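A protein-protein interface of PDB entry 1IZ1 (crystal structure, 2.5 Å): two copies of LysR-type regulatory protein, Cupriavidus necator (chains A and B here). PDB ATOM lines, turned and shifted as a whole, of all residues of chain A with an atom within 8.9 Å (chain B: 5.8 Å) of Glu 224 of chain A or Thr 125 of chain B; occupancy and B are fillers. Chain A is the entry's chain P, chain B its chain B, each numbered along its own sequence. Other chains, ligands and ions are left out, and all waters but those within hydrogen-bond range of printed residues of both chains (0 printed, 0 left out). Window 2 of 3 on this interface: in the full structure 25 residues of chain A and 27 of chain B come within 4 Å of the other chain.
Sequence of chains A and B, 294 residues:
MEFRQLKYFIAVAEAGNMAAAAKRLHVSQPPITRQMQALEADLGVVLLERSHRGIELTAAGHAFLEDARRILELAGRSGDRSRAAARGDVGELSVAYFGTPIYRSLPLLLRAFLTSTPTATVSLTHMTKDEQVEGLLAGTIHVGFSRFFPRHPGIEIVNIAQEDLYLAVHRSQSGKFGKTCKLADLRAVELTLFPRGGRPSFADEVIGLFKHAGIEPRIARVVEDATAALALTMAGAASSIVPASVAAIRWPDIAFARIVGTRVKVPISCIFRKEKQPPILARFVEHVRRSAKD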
ATOM      1  N   PHE A  98     -24.427  -3.050  -4.840  1.00  0.00           N
ATOM      2  CA  PHE A  98     -23.711  -3.238  -3.607  1.00  0.00           C
ATOM      3  C   PHE A  98     -23.170  -4.660  -3.638  1.00  0.00           C
ATOM      4  O   PHE A  98     -23.848  -5.558  -4.119  1.00  0.00           O
ATOM      5  CB  PHE A  98     -24.629  -3.049  -2.400  1.00  0.00           C
ATOM      6  CG  PHE A  98     -23.905  -3.047  -1.081  1.00  0.00           C
ATOM      7  CD1 PHE A  98     -23.114  -1.948  -0.709  1.00  0.00           C
ATOM      8  CD2 PHE A  98     -23.990  -4.142  -0.217  1.00  0.00           C
ATOM      9  CE1 PHE A  98     -22.412  -1.926   0.517  1.00  0.00           C
ATOM     10  CE2 PHE A  98     -23.314  -4.143   1.001  1.00  0.00           C
ATOM     11  CZ  PHE A  98     -22.515  -3.012   1.383  1.00  0.00           C
ATOM     12  N   GLY A  99     -21.933  -4.836  -3.177  1.00  0.00           N
ATOM     13  CA  GLY A  99     -21.329  -6.134  -3.096  1.00  0.00           C
ATOM     14  C   GLY A  99     -20.774  -6.687  -4.393  1.00  0.00           C
ATOM     15  O   GLY A  99     -20.590  -5.997  -5.402  1.00  0.00           O
ATOM     16  N   HIS A 126     -22.210   2.670  -7.226  1.00  0.00           N
ATOM     17  CA  HIS A 126     -22.151   2.003  -5.958  1.00  0.00           C
ATOM     18  C   HIS A 126     -22.964   2.820  -4.967  1.00  0.00           C
ATOM     19  O   HIS A 126     -22.681   3.994  -4.759  1.00  0.00           O
ATOM     20  CB  HIS A 126     -20.720   1.897  -5.444  1.00  0.00           C
ATOM     21  CG  HIS A 126     -20.641   1.359  -4.053  1.00  0.00           C
ATOM     22  ND1 HIS A 126     -20.460   0.015  -3.785  1.00  0.00           N
ATOM     23  CD2 HIS A 126     -20.798   1.969  -2.856  1.00  0.00           C
ATOM     24  CE1 HIS A 126     -20.476  -0.170  -2.477  1.00  0.00           C
ATOM     25  NE2 HIS A 126     -20.681   0.998  -1.891  1.00  0.00           N
ATOM     26  N   THR A 192     -10.820 -13.277   7.031  1.00  0.00           N
ATOM     27  CA  THR A 192     -11.153 -11.879   6.925  1.00  0.00           C
ATOM     28  C   THR A 192     -12.419 -11.816   6.104  1.00  0.00           C
ATOM     29  O   THR A 192     -12.416 -12.167   4.922  1.00  0.00           O
ATOM     30  CB  THR A 192     -10.022 -11.107   6.263  1.00  0.00           C
ATOM     31  OG1 THR A 192      -8.862 -11.146   7.105  1.00  0.00           O
ATOM     32  CG2 THR A 192     -10.381  -9.618   6.129  1.00  0.00           C
ATOM     33  N   LEU A 193     -13.514 -11.429   6.740  1.00  0.00           N
ATOM     34  CA  LEU A 193     -14.783 -11.291   6.035  1.00  0.00           C
ATOM     35  C   LEU A 193     -15.107  -9.830   5.753  1.00  0.00           C
ATOM     36  O   LEU A 193     -14.305  -8.960   6.067  1.00  0.00           O
ATOM     37  CB  LEU A 193     -15.894 -11.992   6.827  1.00  0.00           C
ATOM     38  CG  LEU A 193     -15.619 -13.507   6.888  1.00  0.00           C
ATOM     39  CD1 LEU A 193     -16.569 -14.212   7.848  1.00  0.00           C
ATOM     40  CD2 LEU A 193     -15.723 -14.097   5.478  1.00  0.00           C
ATOM     41  N   PHE A 194     -16.255  -9.593   5.120  1.00  0.00           N
ATOM     42  CA  PHE A 194     -16.712  -8.269   4.687  1.00  0.00           C
ATOM     43  C   PHE A 194     -18.214  -8.360   4.316  1.00  0.00           C
ATOM     44  O   PHE A 194     -18.708  -9.458   4.135  1.00  0.00           O
ATOM     45  CB  PHE A 194     -15.913  -7.858   3.464  1.00  0.00           C
ATOM     46  CG  PHE A 194     -16.042  -8.821   2.337  1.00  0.00           C
ATOM     47  CD1 PHE A 194     -17.067  -8.710   1.435  1.00  0.00           C
ATOM     48  CD2 PHE A 194     -15.173  -9.850   2.206  1.00  0.00           C
ATOM     49  CE1 PHE A 194     -17.203  -9.599   0.422  1.00  0.00           C
ATOM     50  CE2 PHE A 194     -15.312 -10.739   1.219  1.00  0.00           C
ATOM     51  CZ  PHE A 194     -16.334 -10.622   0.319  1.00  0.00           C
ATOM     52  N   PRO A 195     -18.963  -7.256   4.229  1.00  0.00           N
ATOM     53  CA  PRO A 195     -18.591  -5.933   4.757  1.00  0.00           C
ATOM     54  C   PRO A 195     -18.927  -5.765   6.250  1.00  0.00           C
ATOM     55  O   PRO A 195     -19.497  -6.672   6.860  1.00  0.00           O
ATOM     56  CB  PRO A 195     -19.470  -4.993   3.939  1.00  0.00           C
ATOM     57  CG  PRO A 195     -20.723  -5.792   3.702  1.00  0.00           C
ATOM     58  CD  PRO A 195     -20.283  -7.222   3.573  1.00  0.00           C
ATOM     59  N   ARG A 196     -18.568  -4.610   6.811  1.00  0.00           N
ATOM     60  CA  ARG A 196     -18.956  -4.223   8.181  1.00  0.00           C
ATOM     61  C   ARG A 196     -20.413  -3.750   8.177  1.00  0.00           C
ATOM     62  O   ARG A 196     -20.868  -3.133   7.229  1.00  0.00           O
ATOM     63  CB  ARG A 196     -18.027  -3.115   8.747  1.00  0.00           C
ATOM     64  CG  ARG A 196     -16.644  -3.620   9.181  1.00  0.00           C
ATOM     65  CD  ARG A 196     -15.805  -2.690  10.101  1.00  0.00           C
ATOM     66  NE  ARG A 196     -14.818  -1.893   9.338  1.00  0.00           N
ATOM     67  CZ  ARG A 196     -13.470  -2.056   9.342  1.00  0.00           C
ATOM     68  NH1 ARG A 196     -12.883  -3.009  10.075  1.00  0.00           N
ATOM     69  NH2 ARG A 196     -12.697  -1.247   8.612  1.00  0.00           N
ATOM     70  N   GLY A 197     -21.143  -4.091   9.221  1.00  0.00           N
ATOM     71  CA  GLY A 197     -22.490  -3.590   9.430  1.00  0.00           C
ATOM     72  C   GLY A 197     -23.529  -3.438   8.301  1.00  0.00           C
ATOM     73  O   GLY A 197     -24.318  -2.481   8.300  1.00  0.00           O
ATOM     74  N   GLY A 198     -23.612  -4.360   7.360  1.00  0.00           N
ATOM     75  CA  GLY A 198     -24.665  -4.224   6.349  1.00  0.00           C
ATOM     76  C   GLY A 198     -25.845  -5.089   6.727  1.00  0.00           C
ATOM     77  O   GLY A 198     -26.476  -5.711   5.853  1.00  0.00           O
ATOM     78  N   SER A 201     -25.598  -9.130   6.526  1.00  0.00           N
ATOM     79  CA  SER A 201     -24.696  -8.937   5.364  1.00  0.00           C
ATOM     80  C   SER A 201     -24.107 -10.227   4.831  1.00  0.00           C
ATOM     81  O   SER A 201     -24.372 -11.294   5.350  1.00  0.00           O
ATOM     82  CB  SER A 201     -23.523  -8.034   5.770  1.00  0.00           C
ATOM     83  OG  SER A 201     -22.716  -8.627   6.782  1.00  0.00           O
ATOM     84  N   ARG A 221     -11.082 -10.795  11.441  1.00  0.00           N
ATOM     85  CA  ARG A 221     -11.561  -9.419  11.281  1.00  0.00           C
ATOM     86  C   ARG A 221     -12.641  -9.250  10.224  1.00  0.00           C
ATOM     87  O   ARG A 221     -12.853 -10.110   9.391  1.00  0.00           O
ATOM     88  CB  ARG A 221     -10.413  -8.495  10.907  1.00  0.00           C
ATOM     89  CG  ARG A 221      -9.607  -8.938   9.695  1.00  0.00           C
ATOM     90  CD  ARG A 221      -8.490  -7.949   9.369  1.00  0.00           C
ATOM     91  NE  ARG A 221      -7.315  -8.552   8.756  1.00  0.00           N
ATOM     92  CZ  ARG A 221      -6.144  -7.935   8.636  1.00  0.00           C
ATOM     93  NH1 ARG A 221      -5.974  -6.685   9.088  1.00  0.00           N
ATOM     94  NH2 ARG A 221      -5.137  -8.567   8.055  1.00  0.00           N
ATOM     95  N   VAL A 222     -13.306  -8.107  10.259  1.00  0.00           N
ATOM     96  CA  VAL A 222     -14.278  -7.755   9.238  1.00  0.00           C
ATOM     97  C   VAL A 222     -13.905  -6.394   8.650  1.00  0.00           C
ATOM     98  O   VAL A 222     -13.808  -5.396   9.372  1.00  0.00           O
ATOM     99  CB  VAL A 222     -15.717  -7.787   9.788  1.00  0.00           C
ATOM    100  CG1 VAL A 222     -16.723  -7.792   8.668  1.00  0.00           C
ATOM    101  CG2 VAL A 222     -15.912  -9.038  10.645  1.00  0.00           C
ATOM    102  N   VAL A 223     -13.653  -6.387   7.341  1.00  0.00           N
ATOM    103  CA  VAL A 223     -13.147  -5.223   6.644  1.00  0.00           C
ATOM    104  C   VAL A 223     -14.265  -4.628   5.770  1.00  0.00           C
ATOM    105  O   VAL A 223     -15.321  -5.232   5.626  1.00  0.00           O
ATOM    106  CB  VAL A 223     -11.857  -5.572   5.830  1.00  0.00           C
ATOM    107  CG1 VAL A 223     -10.803  -6.092   6.746  1.00  0.00           C
ATOM    108  CG2 VAL A 223     -12.136  -6.574   4.725  1.00  0.00           C
ATOM    109  N   GLU A 224     -14.042  -3.440   5.215  1.00  0.00           N
ATOM    110  CA  GLU A 224     -15.172  -2.674   4.652  1.00  0.00           C
ATOM    111  C   GLU A 224     -15.857  -3.319   3.446  1.00  0.00           C
ATOM    112  O   GLU A 224     -17.066  -3.157   3.290  1.00  0.00           O
ATOM    113  CB  GLU A 224     -14.836  -1.182   4.347  1.00  0.00           C
ATOM    114  CG  GLU A 224     -13.503  -0.857   3.711  1.00  0.00           C
ATOM    115  CD  GLU A 224     -13.374   0.625   3.355  1.00  0.00           C
ATOM    116  OE1 GLU A 224     -13.705   1.468   4.218  1.00  0.00           O
ATOM    117  OE2 GLU A 224     -12.937   0.946   2.225  1.00  0.00           O
ATOM    118  N   ASP A 225     -15.090  -4.050   2.634  1.00  0.00           N
ATOM    119  CA  ASP A 225     -15.598  -4.665   1.410  1.00  0.00           C
ATOM    120  C   ASP A 225     -14.623  -5.681   0.802  1.00  0.00           C
ATOM    121  O   ASP A 225     -13.514  -5.837   1.273  1.00  0.00           O
ATOM    122  CB  ASP A 225     -15.943  -3.593   0.362  1.00  0.00           C
ATOM    123  CG  ASP A 225     -14.759  -2.717  -0.010  1.00  0.00           C
ATOM    124  OD1 ASP A 225     -13.588  -3.026   0.291  1.00  0.00           O
ATOM    125  OD2 ASP A 225     -14.911  -1.667  -0.647  1.00  0.00           O
ATOM    126  N   ALA A 226     -15.037  -6.330  -0.279  1.00  0.00           N
ATOM    127  CA  ALA A 226     -14.229  -7.390  -0.919  1.00  0.00           C
ATOM    128  C   ALA A 226     -12.922  -6.895  -1.417  1.00  0.00           C
ATOM    129  O   ALA A 226     -11.972  -7.660  -1.452  1.00  0.00           O
ATOM    130  CB  ALA A 226     -14.969  -8.044  -2.077  1.00  0.00           C
ATOM    131  N   THR A 227     -12.879  -5.630  -1.821  1.00  0.00           N
ATOM    132  CA  THR A 227     -11.647  -5.015  -2.258  1.00  0.00           C
ATOM    133  C   THR A 227     -10.573  -5.126  -1.190  1.00  0.00           C
ATOM    134  O   THR A 227      -9.447  -5.529  -1.502  1.00  0.00           O
ATOM    135  CB  THR A 227     -11.846  -3.544  -2.646  1.00  0.00           C
ATOM    136  OG1 THR A 227     -12.614  -3.460  -3.854  1.00  0.00           O
ATOM    137  CG2 THR A 227     -10.502  -2.900  -3.024  1.00  0.00           C
ATOM    138  N   ALA A 228     -10.919  -4.789   0.054  1.00  0.00           N
ATOM    139  CA  ALA A 228      -9.947  -4.769   1.135  1.00  0.00           C
ATOM    140  C   ALA A 228      -9.482  -6.181   1.478  1.00  0.00           C
ATOM    141  O   ALA A 228      -8.309  -6.431   1.558  1.00  0.00           O
ATOM    142  CB  ALA A 228     -10.522  -4.099   2.359  1.00  0.00           C
ATOM    143  N   ALA A 229     -10.413  -7.101   1.686  1.00  0.00           N
ATOM    144  CA  ALA A 229     -10.053  -8.488   1.939  1.00  0.00           C
ATOM    145  C   ALA A 229      -9.208  -9.132   0.798  1.00  0.00           C
ATOM    146  O   ALA A 229      -8.276  -9.885   1.067  1.00  0.00           O
ATOM    147  CB  ALA A 229     -11.291  -9.293   2.222  1.00  0.00           C
ATOM    148  N   LEU A 232      -5.672  -7.658   1.073  1.00  0.00           N
ATOM    149  CA  LEU A 232      -4.962  -8.223   2.188  1.00  0.00           C
ATOM    150  C   LEU A 232      -4.591  -9.662   1.875  1.00  0.00           C
ATOM    151  O   LEU A 232      -3.528 -10.112   2.235  1.00  0.00           O
ATOM    152  CB  LEU A 232      -5.822  -8.160   3.433  1.00  0.00           C
ATOM    153  CG  LEU A 232      -6.097  -6.773   4.020  1.00  0.00           C
ATOM    154  CD1 LEU A 232      -7.147  -6.856   5.101  1.00  0.00           C
ATOM    155  CD2 LEU A 232      -4.829  -6.171   4.566  1.00  0.00           C
ATOM    156  N   SER B  94      -2.516   2.438   9.757  1.00  0.00           N
ATOM    157  CA  SER B  94      -3.791   2.804   9.171  1.00  0.00           C
ATOM    158  C   SER B  94      -3.534   3.416   7.791  1.00  0.00           C
ATOM    159  O   SER B  94      -2.864   4.421   7.669  1.00  0.00           O
ATOM    160  CB  SER B  94      -4.479   3.821  10.093  1.00  0.00           C
ATOM    161  OG  SER B  94      -5.829   4.085   9.732  1.00  0.00           O
ATOM    162  N   VAL B  95      -4.070   2.783   6.762  1.00  0.00           N
ATOM    163  CA  VAL B  95      -3.770   3.094   5.366  1.00  0.00           C
ATOM    164  C   VAL B  95      -5.052   3.402   4.623  1.00  0.00           C
ATOM    165  O   VAL B  95      -6.076   2.727   4.825  1.00  0.00           O
ATOM    166  CB  VAL B  95      -3.182   1.890   4.692  1.00  0.00           C
ATOM    167  CG1 VAL B  95      -2.980   2.152   3.217  1.00  0.00           C
ATOM    168  CG2 VAL B  95      -1.875   1.494   5.392  1.00  0.00           C
ATOM    169  N   ALA B  96      -5.011   4.422   3.781  1.00  0.00           N
ATOM    170  CA  ALA B  96      -6.119   4.704   2.896  1.00  0.00           C
ATOM    171  C   ALA B  96      -5.663   4.709   1.457  1.00  0.00           C
ATOM    172  O   ALA B  96      -4.497   4.878   1.145  1.00  0.00           O
ATOM    173  CB  ALA B  96      -6.762   6.032   3.245  1.00  0.00           C
ATOM    174  N   TYR B  97      -6.638   4.529   0.580  1.00  0.00           N
ATOM    175  CA  TYR B  97      -6.390   4.464  -0.837  1.00  0.00           C
ATOM    176  C   TYR B  97      -7.542   5.064  -1.622  1.00  0.00           C
ATOM    177  O   TYR B  97      -8.688   5.043  -1.194  1.00  0.00           O
ATOM    178  CB  TYR B  97      -6.162   3.021  -1.257  1.00  0.00           C
ATOM    179  CG  TYR B  97      -7.397   2.150  -1.164  1.00  0.00           C
ATOM    180  CD1 TYR B  97      -8.228   1.957  -2.263  1.00  0.00           C
ATOM    181  CD2 TYR B  97      -7.733   1.510   0.028  1.00  0.00           C
ATOM    182  CE1 TYR B  97      -9.373   1.138  -2.177  1.00  0.00           C
ATOM    183  CE2 TYR B  97      -8.863   0.699   0.120  1.00  0.00           C
ATOM    184  CZ  TYR B  97      -9.671   0.518  -0.980  1.00  0.00           C
ATOM    185  OH  TYR B  97     -10.784  -0.260  -0.867  1.00  0.00           O
ATOM    186  N   PHE B  98      -7.191   5.603  -2.780  1.00  0.00           N
ATOM    187  CA  PHE B  98      -8.124   5.925  -3.850  1.00  0.00           C
ATOM    188  C   PHE B  98      -7.577   5.329  -5.163  1.00  0.00           C
ATOM    189  O   PHE B  98      -6.348   5.243  -5.361  1.00  0.00           O
ATOM    190  CB  PHE B  98      -8.236   7.440  -3.972  1.00  0.00           C
ATOM    191  CG  PHE B  98      -9.377   7.909  -4.838  1.00  0.00           C
ATOM    192  CD1 PHE B  98     -10.698   7.670  -4.469  1.00  0.00           C
ATOM    193  CD2 PHE B  98      -9.124   8.617  -6.040  1.00  0.00           C
ATOM    194  CE1 PHE B  98     -11.742   8.124  -5.269  1.00  0.00           C
ATOM    195  CE2 PHE B  98     -10.162   9.067  -6.840  1.00  0.00           C
ATOM    196  CZ  PHE B  98     -11.464   8.830  -6.460  1.00  0.00           C
ATOM    197  N   SER B 123      -4.756  -1.717   8.431  1.00  0.00           N
ATOM    198  CA  SER B 123      -6.162  -1.625   8.074  1.00  0.00           C
ATOM    199  C   SER B 123      -6.275  -0.774   6.834  1.00  0.00           C
ATOM    200  O   SER B 123      -5.490   0.134   6.632  1.00  0.00           O
ATOM    201  CB  SER B 123      -6.964  -1.027   9.208  1.00  0.00           C
ATOM    202  OG  SER B 123      -6.455   0.240   9.502  1.00  0.00           O
ATOM    203  N   LEU B 124      -7.252  -1.080   5.997  1.00  0.00           N
ATOM    204  CA  LEU B 124      -7.401  -0.416   4.721  1.00  0.00           C
ATOM    205  C   LEU B 124      -8.737   0.321   4.646  1.00  0.00           C
ATOM    206  O   LEU B 124      -9.761  -0.182   5.096  1.00  0.00           O
ATOM    207  CB  LEU B 124      -7.310  -1.452   3.606  1.00  0.00           C
ATOM    208  CG  LEU B 124      -5.888  -1.734   3.141  1.00  0.00           C
ATOM    209  CD1 LEU B 124      -5.764  -3.156   2.567  1.00  0.00           C
ATOM    210  CD2 LEU B 124      -5.483  -0.687   2.102  1.00  0.00           C
ATOM    211  N   THR B 125      -8.722   1.502   4.050  1.00  0.00           N
ATOM    212  CA  THR B 125      -9.932   2.292   3.903  1.00  0.00           C
ATOM    213  C   THR B 125      -9.938   3.016   2.586  1.00  0.00           C
ATOM    214  O   THR B 125      -9.052   3.824   2.340  1.00  0.00           O
ATOM    215  CB  THR B 125     -10.049   3.356   5.004  1.00  0.00           C
ATOM    216  OG1 THR B 125      -9.650   2.795   6.244  1.00  0.00           O
ATOM    217  CG2 THR B 125     -11.520   3.748   5.223  1.00  0.00           C
ATOM    218  N   HIS B 126     -10.944   2.747   1.755  1.00  0.00           N
ATOM    219  CA  HIS B 126     -11.240   3.644   0.656  1.00  0.00           C
ATOM    220  C   HIS B 126     -11.448   5.078   1.158  1.00  0.00           C
ATOM    221  O   HIS B 126     -12.103   5.313   2.144  1.00  0.00           O
ATOM    222  CB  HIS B 126     -12.448   3.209  -0.172  1.00  0.00           C
ATOM    223  CG  HIS B 126     -12.637   4.059  -1.390  1.00  0.00           C
ATOM    224  ND1 HIS B 126     -11.905   3.876  -2.547  1.00  0.00           N
ATOM    225  CD2 HIS B 126     -13.404   5.156  -1.597  1.00  0.00           C
ATOM    226  CE1 HIS B 126     -12.246   4.799  -3.426  1.00  0.00           C
ATOM    227  NE2 HIS B 126     -13.145   5.592  -2.870  1.00  0.00           N
ATOM    228  N   MET B 127     -10.879   6.029   0.446  1.00  0.00           N
ATOM    229  CA  MET B 127     -10.940   7.420   0.833  1.00  0.00           C
ATOM    230  C   MET B 127     -10.632   8.353  -0.354  1.00  0.00           C
ATOM    231  O   MET B 127      -9.664   8.158  -1.099  1.00  0.00           O
ATOM    232  CB  MET B 127      -9.954   7.629   1.949  1.00  0.00           C
ATOM    233  CG  MET B 127     -10.549   8.279   3.138  1.00  0.00           C
ATOM    234  SD  MET B 127      -9.417   8.546   4.512  1.00  0.00           S
ATOM    235  CE  MET B 127     -10.341   7.723   5.792  1.00  0.00           C
ATOM    236  N   ILE B 141      -5.621   8.427  10.065  1.00  0.00           N
ATOM    237  CA  ILE B 141      -4.890   7.534   9.176  1.00  0.00           C
ATOM    238  C   ILE B 141      -3.421   7.966   9.132  1.00  0.00           C
ATOM    239  O   ILE B 141      -3.124   9.146   9.384  1.00  0.00           O
ATOM    240  CB  ILE B 141      -5.510   7.508   7.760  1.00  0.00           C
ATOM    241  CG1 ILE B 141      -5.680   8.901   7.196  1.00  0.00           C
ATOM    242  CG2 ILE B 141      -6.865   6.811   7.748  1.00  0.00           C
ATOM    243  CD1 ILE B 141      -5.422   8.967   5.702  1.00  0.00           C
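OE2 of Glu 224 of chain A lies within hydrogen-bond range of N of His 126 of chain B, at 2.7 Å.
O of Val 95 of chain B is in hydrogen-bond range of N of Thr 125 of chain B. The backbone carbonyl oxygen (O) of Thr 125 of chain B sits at hydrogen-bond distance from the backbone NH (N) of Tyr 97 of chain B (3.1 Å). The backbone carbonyl oxygen (O) of Tyr 97 of chain B sits at hydrogen-bond distance from the backbone NH (N) of Met 127 of chain B. OD1 of Asp 225 of chain A sits close to N of Thr 227 of chain A.
Among the printed residues, merely in contact across the chains: Glu 224 of chain A with Thr 125 of chain B (3.3 Å), Thr 227 of chain A with Tyr 97 of chain B (3.4 Å), Leu 232 of chain A with Leu 124 of chain B (3.7 Å) and Glu 224 of chain A with Tyr 97 of chain B (3.96 Å).
Gly 197 of chain A touches none of the printed residues of chain B. Of the printed residues of chain B, Thr 227 of chain A touches Tyr 97. Printed residues of chain B within 4 Å of Leu 232 of chain A: Leu 124. No residue of chain A comes within 4 Å of Ala 96 of chain B. Printed residues of chain A within 4 Å of Thr 125 of chain B: Glu 224. Of the printed residues of chain A, His 126 of chain B touches Glu 224 (2.7 Å).
Of the 11 printed residues of chain B, 4 touch a printed residue of chain A.
Positions printed for both chains: 98 and 126.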
